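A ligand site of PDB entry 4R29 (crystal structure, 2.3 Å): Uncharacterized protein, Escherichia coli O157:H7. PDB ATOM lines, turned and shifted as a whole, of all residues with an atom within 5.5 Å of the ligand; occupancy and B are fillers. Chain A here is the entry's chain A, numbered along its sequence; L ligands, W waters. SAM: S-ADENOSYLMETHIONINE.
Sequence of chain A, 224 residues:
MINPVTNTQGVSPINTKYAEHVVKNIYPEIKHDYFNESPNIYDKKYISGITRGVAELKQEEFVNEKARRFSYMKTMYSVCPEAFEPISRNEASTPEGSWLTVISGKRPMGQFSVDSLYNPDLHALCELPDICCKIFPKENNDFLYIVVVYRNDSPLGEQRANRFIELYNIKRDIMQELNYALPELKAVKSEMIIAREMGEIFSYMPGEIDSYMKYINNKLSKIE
Residues that only touch the ligand: Arg 89 (3.2 Å), Gly 110 (3.4 Å), Ala 195 (3.4 Å), Met 198 (3.6 Å), Gly 199 (3.7 Å), Phe 202 (3.4 Å), Ile 209 (3.9 Å) and Tyr 212 (3.5 Å).
Hydrophobic or aromatic side chains within 4 Å of the ligand: Ala 92, Ala 195, Met 198, Phe 202, Tyr 204 and Tyr 212.
Of the 21 residues printed, 15 come within 4 Å of the ligand.
The guanidinium group (NH1) of Arg 89 lies within hydrogen-bond range of the side-chain hydroxyl (OH) of Tyr 204, 3.2 Å away.
The side-chain carboxylate of Glu 191 is in hydrogen-bond range of the side-chain hydroxyl of Tyr 212.
NH2 of Arg 107 sits at hydrogen-bond distance from O of Ser 98.
The side-chain carboxylate (OE1) of Glu 208 sits at hydrogen-bond distance from the backbone NH (N) of Arg 89, 2.7 Å away.
The backbone carbonyl oxygen (O) of Thr 94 sits at hydrogen-bond distance from the side-chain hydroxyl (OG) of Ser 98, 2.6 Å away.
O of Met 109 sits close to NE of Arg 107 (3.3 Å).
The guanidinium group (NH1) of Arg 107 sits at hydrogen-bond distance from the backbone carbonyl oxygen (O) of Phe 202, 2.9 Å away.
The side-chain hydroxyl (OG) of Ser 98 is in hydrogen-bond range of the backbone carbonyl oxygen (O) of Ala 92 (3.3 Å).
Water W2 lies within hydrogen-bond range of the side-chain carboxylate (OE1) of Glu 191 and an oxygen (O3') of the ligand.
The guanidinium group (NH2) of Arg 107 lies within salt-bridge range of an oxygen (OXT) of the ligand, at 2.6 Å.
OG of Ser 98 is in hydrogen-bond range of N of the ligand (2.6 Å).
An oxygen (O) of the ligand sits at hydrogen-bond distance from the side-chain hydroxyl of Tyr 204 (2.7 Å).
O of Gln 111 sits at hydrogen-bond distance from N of the ligand, 2.6 Å away.
OE2 of Glu 191 is in hydrogen-bond range of O2' of the ligand, 2.5 Å away.
The backbone NH (N) of Gln 111 is in hydrogen-bond range of an oxygen (OXT) of the ligand (3.0 Å).
O of Glu 208 sits at hydrogen-bond distance from N6 of the ligand (3.0 Å).
The backbone carbonyl oxygen of Ala 92 is in hydrogen-bond range of a nitrogen (N) of the ligand (3.2 Å).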
ATOM      1  N   ARG A  89      20.165  -4.271  29.903  1.00  0.00           N
ATOM      2  CA  ARG A  89      19.816  -5.482  30.621  1.00  0.00           C
ATOM      3  C   ARG A  89      19.793  -5.268  32.145  1.00  0.00           C
ATOM      4  O   ARG A  89      18.998  -5.893  32.853  1.00  0.00           O
ATOM      5  CB  ARG A  89      20.839  -6.577  30.257  1.00  0.00           C
ATOM      6  CG  ARG A  89      21.176  -7.535  31.387  1.00  0.00           C
ATOM      7  CD  ARG A  89      20.017  -8.479  31.594  1.00  0.00           C
ATOM      8  NE  ARG A  89      20.185  -9.331  32.765  1.00  0.00           N
ATOM      9  CZ  ARG A  89      19.221 -10.118  33.242  1.00  0.00           C
ATOM     10  NH1 ARG A  89      18.035 -10.120  32.648  1.00  0.00           N
ATOM     11  NH2 ARG A  89      19.450 -10.869  34.304  1.00  0.00           N
ATOM     12  N   ALA A  92      16.539  -4.350  33.932  1.00  0.00           N
ATOM     13  CA  ALA A  92      15.483  -5.352  33.972  1.00  0.00           C
ATOM     14  C   ALA A  92      15.980  -6.691  34.497  1.00  0.00           C
ATOM     15  O   ALA A  92      15.508  -7.736  34.074  1.00  0.00           O
ATOM     16  CB  ALA A  92      14.863  -5.520  32.594  1.00  0.00           C
ATOM     17  N   SER A  93      16.931  -6.656  35.415  1.00  0.00           N
ATOM     18  CA  SER A  93      17.506  -7.893  35.928  1.00  0.00           C
ATOM     19  C   SER A  93      16.856  -8.344  37.227  1.00  0.00           C
ATOM     20  O   SER A  93      17.152  -9.427  37.711  1.00  0.00           O
ATOM     21  CB  SER A  93      19.020  -7.743  36.145  1.00  0.00           C
ATOM     22  OG  SER A  93      19.291  -6.695  37.057  1.00  0.00           O
ATOM     23  N   THR A  94      15.975  -7.520  37.797  1.00  0.00           N
ATOM     24  CA  THR A  94      15.182  -7.922  38.951  1.00  0.00           C
ATOM     25  C   THR A  94      13.731  -8.005  38.515  1.00  0.00           C
ATOM     26  O   THR A  94      13.357  -7.459  37.473  1.00  0.00           O
ATOM     27  CB  THR A  94      15.333  -6.927  40.131  1.00  0.00           C
ATOM     28  OG1 THR A  94      14.785  -5.646  39.782  1.00  0.00           O
ATOM     29  CG2 THR A  94      16.811  -6.763  40.520  1.00  0.00           C
ATOM     30  N   SER A  98      11.962  -5.435  35.788  1.00  0.00           N
ATOM     31  CA  SER A  98      11.373  -6.119  34.652  1.00  0.00           C
ATOM     32  C   SER A  98      10.045  -5.499  34.243  1.00  0.00           C
ATOM     33  O   SER A  98       9.789  -5.321  33.062  1.00  0.00           O
ATOM     34  CB  SER A  98      11.204  -7.616  34.924  1.00  0.00           C
ATOM     35  OG  SER A  98      12.458  -8.240  35.159  1.00  0.00           O
ATOM     36  N   ARG A 107      10.028   0.184  27.226  1.00  0.00           N
ATOM     37  CA  ARG A 107      10.003  -0.929  26.281  1.00  0.00           C
ATOM     38  C   ARG A 107       8.613  -1.572  26.295  1.00  0.00           C
ATOM     39  O   ARG A 107       7.843  -1.375  27.221  1.00  0.00           O
ATOM     40  CB  ARG A 107      11.097  -1.978  26.617  1.00  0.00           C
ATOM     41  CG  ARG A 107      10.983  -2.598  28.002  1.00  0.00           C
ATOM     42  CD  ARG A 107      12.015  -3.712  28.236  1.00  0.00           C
ATOM     43  NE  ARG A 107      11.792  -4.356  29.522  1.00  0.00           N
ATOM     44  CZ  ARG A 107      12.186  -5.589  29.846  1.00  0.00           C
ATOM     45  NH1 ARG A 107      12.860  -6.350  28.963  1.00  0.00           N
ATOM     46  NH2 ARG A 107      11.920  -6.060  31.047  1.00  0.00           N
ATOM     47  N   MET A 109       7.718  -4.985  26.300  1.00  0.00           N
ATOM     48  CA  MET A 109       7.486  -6.135  27.178  1.00  0.00           C
ATOM     49  C   MET A 109       8.670  -6.599  28.020  1.00  0.00           C
ATOM     50  O   MET A 109       9.829  -6.262  27.765  1.00  0.00           O
ATOM     51  CB  MET A 109       6.773  -7.321  26.485  1.00  0.00           C
ATOM     52  CG  MET A 109       7.593  -8.386  25.870  1.00  0.00           C
ATOM     53  SD  MET A 109       8.467  -9.619  26.902  1.00  0.00           S
ATOM     54  CE  MET A 109       9.558 -10.128  25.566  1.00  0.00           C
ATOM     55  N   GLY A 110       8.318  -7.298  29.101  1.00  0.00           N
ATOM     56  CA  GLY A 110       9.274  -7.834  30.047  1.00  0.00           C
ATOM     57  C   GLY A 110       8.685  -9.120  30.603  1.00  0.00           C
ATOM     58  O   GLY A 110       7.497  -9.401  30.420  1.00  0.00           O
ATOM     59  N   GLN A 111       9.512  -9.912  31.269  1.00  0.00           N
ATOM     60  CA  GLN A 111       9.091 -11.191  31.803  1.00  0.00           C
ATOM     61  C   GLN A 111       9.748 -11.346  33.171  1.00  0.00           C
ATOM     62  O   GLN A 111      10.902 -10.983  33.343  1.00  0.00           O
ATOM     63  CB  GLN A 111       9.475 -12.337  30.837  1.00  0.00           C
ATOM     64  CG  GLN A 111       9.232 -13.750  31.385  1.00  0.00           C
ATOM     65  CD  GLN A 111      10.390 -14.256  32.249  1.00  0.00           C
ATOM     66  OE1 GLN A 111      11.541 -14.157  31.856  1.00  0.00           O
ATOM     67  NE2 GLN A 111      10.073 -14.797  33.406  1.00  0.00           N
ATOM     68  N   PHE A 112       9.010 -11.836  34.147  1.00  0.00           N
ATOM     69  CA  PHE A 112       9.553 -12.092  35.479  1.00  0.00           C
ATOM     70  C   PHE A 112       8.815 -13.267  36.106  1.00  0.00           C
ATOM     71  O   PHE A 112       7.963 -13.868  35.472  1.00  0.00           O
ATOM     72  CB  PHE A 112       9.494 -10.816  36.349  1.00  0.00           C
ATOM     73  CG  PHE A 112       8.092 -10.289  36.597  1.00  0.00           C
ATOM     74  CD1 PHE A 112       7.475  -9.445  35.676  1.00  0.00           C
ATOM     75  CD2 PHE A 112       7.406 -10.612  37.765  1.00  0.00           C
ATOM     76  CE1 PHE A 112       6.192  -8.934  35.912  1.00  0.00           C
ATOM     77  CE2 PHE A 112       6.126 -10.110  38.024  1.00  0.00           C
ATOM     78  CZ  PHE A 112       5.513  -9.269  37.075  1.00  0.00           C
ATOM     79  N   GLU A 191      20.166 -22.174  25.377  1.00  0.00           N
ATOM     80  CA  GLU A 191      20.451 -20.735  25.312  1.00  0.00           C
ATOM     81  C   GLU A 191      21.096 -20.345  23.989  1.00  0.00           C
ATOM     82  O   GLU A 191      20.821 -19.259  23.464  1.00  0.00           O
ATOM     83  CB  GLU A 191      21.374 -20.306  26.457  1.00  0.00           C
ATOM     84  CG  GLU A 191      20.681 -20.183  27.822  1.00  0.00           C
ATOM     85  CD  GLU A 191      19.498 -19.217  27.803  1.00  0.00           C
ATOM     86  OE1 GLU A 191      18.355 -19.688  27.706  1.00  0.00           O
ATOM     87  OE2 GLU A 191      19.706 -17.998  27.911  1.00  0.00           O
ATOM     88  N   ILE A 194      18.210 -19.805  21.447  1.00  0.00           N
ATOM     89  CA  ILE A 194      17.187 -18.746  21.513  1.00  0.00           C
ATOM     90  C   ILE A 194      17.597 -17.441  22.206  1.00  0.00           C
ATOM     91  O   ILE A 194      16.819 -16.496  22.228  1.00  0.00           O
ATOM     92  CB  ILE A 194      15.895 -19.271  22.160  1.00  0.00           C
ATOM     93  CG1 ILE A 194      16.196 -19.998  23.465  1.00  0.00           C
ATOM     94  CG2 ILE A 194      15.138 -20.176  21.185  1.00  0.00           C
ATOM     95  CD1 ILE A 194      16.309 -19.111  24.664  1.00  0.00           C
ATOM     96  N   ALA A 195      18.806 -17.388  22.755  1.00  0.00           N
ATOM     97  CA  ALA A 195      19.164 -16.291  23.646  1.00  0.00           C
ATOM     98  C   ALA A 195      19.222 -14.943  22.921  1.00  0.00           C
ATOM     99  O   ALA A 195      18.743 -13.956  23.438  1.00  0.00           O
ATOM    100  CB  ALA A 195      20.484 -16.573  24.390  1.00  0.00           C
ATOM    101  N   ARG A 196      19.821 -14.903  21.730  1.00  0.00           N
ATOM    102  CA  ARG A 196      19.909 -13.660  20.968  1.00  0.00           C
ATOM    103  C   ARG A 196      18.527 -13.155  20.590  1.00  0.00           C
ATOM    104  O   ARG A 196      18.226 -11.963  20.712  1.00  0.00           O
ATOM    105  CB  ARG A 196      20.755 -13.830  19.699  1.00  0.00           C
ATOM    106  CG  ARG A 196      20.766 -12.581  18.812  1.00  0.00           C
ATOM    107  CD  ARG A 196      21.812 -12.646  17.689  1.00  0.00           C
ATOM    108  NE  ARG A 196      23.176 -12.796  18.184  1.00  0.00           N
ATOM    109  CZ  ARG A 196      23.978 -11.797  18.540  1.00  0.00           C
ATOM    110  NH1 ARG A 196      23.566 -10.542  18.506  1.00  0.00           N
ATOM    111  NH2 ARG A 196      25.209 -12.070  18.971  1.00  0.00           N
ATOM    112  N   MET A 198      15.755 -13.778  22.266  1.00  0.00           N
ATOM    113  CA  MET A 198      15.200 -13.218  23.497  1.00  0.00           C
ATOM    114  C   MET A 198      15.749 -11.823  23.807  1.00  0.00           C
ATOM    115  O   MET A 198      14.980 -10.942  24.166  1.00  0.00           O
ATOM    116  CB  MET A 198      15.537 -14.086  24.698  1.00  0.00           C
ATOM    117  CG  MET A 198      15.223 -15.530  24.531  1.00  0.00           C
ATOM    118  SD  MET A 198      13.959 -15.996  25.707  1.00  0.00           S
ATOM    119  CE  MET A 198      12.682 -14.945  24.995  1.00  0.00           C
ATOM    120  N   GLY A 199      17.061 -11.660  23.717  1.00  0.00           N
ATOM    121  CA  GLY A 199      17.674 -10.387  24.010  1.00  0.00           C
ATOM    122  C   GLY A 199      17.006  -9.275  23.202  1.00  0.00           C
ATOM    123  O   GLY A 199      16.661  -8.206  23.722  1.00  0.00           O
ATOM    124  N   PHE A 202      13.469  -8.481  24.353  1.00  0.00           N
ATOM    125  CA  PHE A 202      13.529  -7.780  25.625  1.00  0.00           C
ATOM    126  C   PHE A 202      14.152  -6.393  25.494  1.00  0.00           C
ATOM    127  O   PHE A 202      14.309  -5.707  26.501  1.00  0.00           O
ATOM    128  CB  PHE A 202      14.297  -8.598  26.671  1.00  0.00           C
ATOM    129  CG  PHE A 202      13.548  -9.802  27.213  1.00  0.00           C
ATOM    130  CD1 PHE A 202      12.264  -9.661  27.718  1.00  0.00           C
ATOM    131  CD2 PHE A 202      14.136 -11.061  27.207  1.00  0.00           C
ATOM    132  CE1 PHE A 202      11.585 -10.765  28.224  1.00  0.00           C
ATOM    133  CE2 PHE A 202      13.459 -12.167  27.700  1.00  0.00           C
ATOM    134  CZ  PHE A 202      12.172 -12.009  28.202  1.00  0.00           C
ATOM    135  N   TYR A 204      17.202  -5.433  24.914  1.00  0.00           N
ATOM    136  CA  TYR A 204      18.523  -5.208  25.471  1.00  0.00           C
ATOM    137  C   TYR A 204      19.377  -4.573  24.398  1.00  0.00           C
ATOM    138  O   TYR A 204      19.112  -4.701  23.207  1.00  0.00           O
ATOM    139  CB  TYR A 204      19.164  -6.521  25.906  1.00  0.00           C
ATOM    140  CG  TYR A 204      18.445  -7.235  27.011  1.00  0.00           C
ATOM    141  CD1 TYR A 204      17.490  -6.591  27.787  1.00  0.00           C
ATOM    142  CD2 TYR A 204      18.712  -8.577  27.284  1.00  0.00           C
ATOM    143  CE1 TYR A 204      16.830  -7.266  28.804  1.00  0.00           C
ATOM    144  CE2 TYR A 204      18.065  -9.250  28.295  1.00  0.00           C
ATOM    145  CZ  TYR A 204      17.126  -8.584  29.043  1.00  0.00           C
ATOM    146  OH  TYR A 204      16.484  -9.252  30.047  1.00  0.00           O
ATOM    147  N   GLU A 208      25.145  -5.674  24.766  1.00  0.00           N
ATOM    148  CA  GLU A 208      24.928  -6.580  25.889  1.00  0.00           C
ATOM    149  C   GLU A 208      24.529  -7.984  25.421  1.00  0.00           C
ATOM    150  O   GLU A 208      24.894  -8.972  26.049  1.00  0.00           O
ATOM    151  CB  GLU A 208      23.874  -6.026  26.832  1.00  0.00           C
ATOM    152  CG  GLU A 208      24.310  -4.710  27.478  1.00  0.00           C
ATOM    153  CD  GLU A 208      23.243  -4.150  28.376  1.00  0.00           C
ATOM    154  OE1 GLU A 208      22.049  -4.343  28.033  1.00  0.00           O
ATOM    155  OE2 GLU A 208      23.585  -3.537  29.406  1.00  0.00           O
ATOM    156  N   ILE A 209      23.803  -8.044  24.320  1.00  0.00           N
ATOM    157  CA  ILE A 209      23.420  -9.323  23.736  1.00  0.00           C
ATOM    158  C   ILE A 209      24.643 -10.079  23.183  1.00  0.00           C
ATOM    159  O   ILE A 209      24.793 -11.289  23.408  1.00  0.00           O
ATOM    160  CB  ILE A 209      22.339  -9.140  22.646  1.00  0.00           C
ATOM    161  CG1 ILE A 209      21.097  -8.422  23.199  1.00  0.00           C
ATOM    162  CG2 ILE A 209      21.978 -10.495  22.042  1.00  0.00           C
ATOM    163  CD1 ILE A 209      20.095  -7.961  22.095  1.00  0.00           C
ATOM    164  N   TYR A 212      26.507 -11.501  25.924  1.00  0.00           N
ATOM    165  CA  TYR A 212      25.871 -12.691  26.515  1.00  0.00           C
ATOM    166  C   TYR A 212      26.105 -13.939  25.645  1.00  0.00           C
ATOM    167  O   TYR A 212      26.334 -15.025  26.171  1.00  0.00           O
ATOM    168  CB  TYR A 212      24.392 -12.459  26.779  1.00  0.00           C
ATOM    169  CG  TYR A 212      23.677 -13.622  27.443  1.00  0.00           C
ATOM    170  CD1 TYR A 212      23.630 -13.742  28.829  1.00  0.00           C
ATOM    171  CD2 TYR A 212      23.060 -14.597  26.694  1.00  0.00           C
ATOM    172  CE1 TYR A 212      22.962 -14.811  29.441  1.00  0.00           C
ATOM    173  CE2 TYR A 212      22.390 -15.657  27.284  1.00  0.00           C
ATOM    174  CZ  TYR A 212      22.340 -15.744  28.652  1.00  0.00           C
ATOM    175  OH  TYR A 212      21.682 -16.810  29.216  1.00  0.00           O
HETATM  176  N   SAM L   1      13.392 -10.139  33.579  1.00  0.00           N
HETATM  177  CA  SAM L   1      14.010 -10.039  32.263  1.00  0.00           C
HETATM  178  C   SAM L   1      13.323  -8.981  31.400  1.00  0.00           C
HETATM  179  O   SAM L   1      13.935  -8.488  30.437  1.00  0.00           O
HETATM  180  OXT SAM L   1      12.168  -8.618  31.638  1.00  0.00           O
HETATM  181  CB  SAM L   1      13.970 -11.358  31.499  1.00  0.00           C
HETATM  182  CG  SAM L   1      14.916 -12.429  32.025  1.00  0.00           C
HETATM  183  SD  SAM L   1      15.255 -13.762  30.826  1.00  0.00           S
HETATM  184  CE  SAM L   1      16.401 -14.683  31.888  1.00  0.00           C
HETATM  185  C5' SAM L   1      16.477 -12.937  29.785  1.00  0.00           C
HETATM  186  C4' SAM L   1      16.904 -13.844  28.639  1.00  0.00           C
HETATM  187  O4' SAM L   1      17.428 -13.074  27.575  1.00  0.00           O
HETATM  188  C3' SAM L   1      17.980 -14.834  29.054  1.00  0.00           C
HETATM  189  O3' SAM L   1      17.421 -16.067  29.473  1.00  0.00           O
HETATM  190  C2' SAM L   1      18.820 -14.985  27.811  1.00  0.00           C
HETATM  191  O2' SAM L   1      18.311 -16.088  27.109  1.00  0.00           O
HETATM  192  C1' SAM L   1      18.534 -13.738  26.985  1.00  0.00           C
HETATM  193  N9  SAM L   1      19.626 -12.738  26.993  1.00  0.00           N
HETATM  194  C8  SAM L   1      20.229 -12.203  25.888  1.00  0.00           C
HETATM  195  N7  SAM L   1      21.153 -11.308  26.277  1.00  0.00           N
HETATM  196  C5  SAM L   1      21.150 -11.267  27.634  1.00  0.00           C
HETATM  197  C6  SAM L   1      21.891 -10.523  28.541  1.00  0.00           C
HETATM  198  N6  SAM L   1      22.807  -9.662  28.108  1.00  0.00           N
HETATM  199  N1  SAM L   1      21.669 -10.687  29.886  1.00  0.00           N
HETATM  200  C2  SAM L   1      20.702 -11.578  30.322  1.00  0.00           C
HETATM  201  N3  SAM L   1      19.963 -12.315  29.421  1.00  0.00           N
HETATM  202  C4  SAM L   1      20.177 -12.163  28.090  1.00  0.00           C
HETATM  203  O   HOH W   1      25.088  -8.219  29.868  1.00  0.00           O
HETATM  204  O   HOH W   2      16.342 -18.121  28.026  1.00  0.00           O
HETATM  205  O   HOH W   3      23.578 -10.143  31.668  1.00  0.00           O
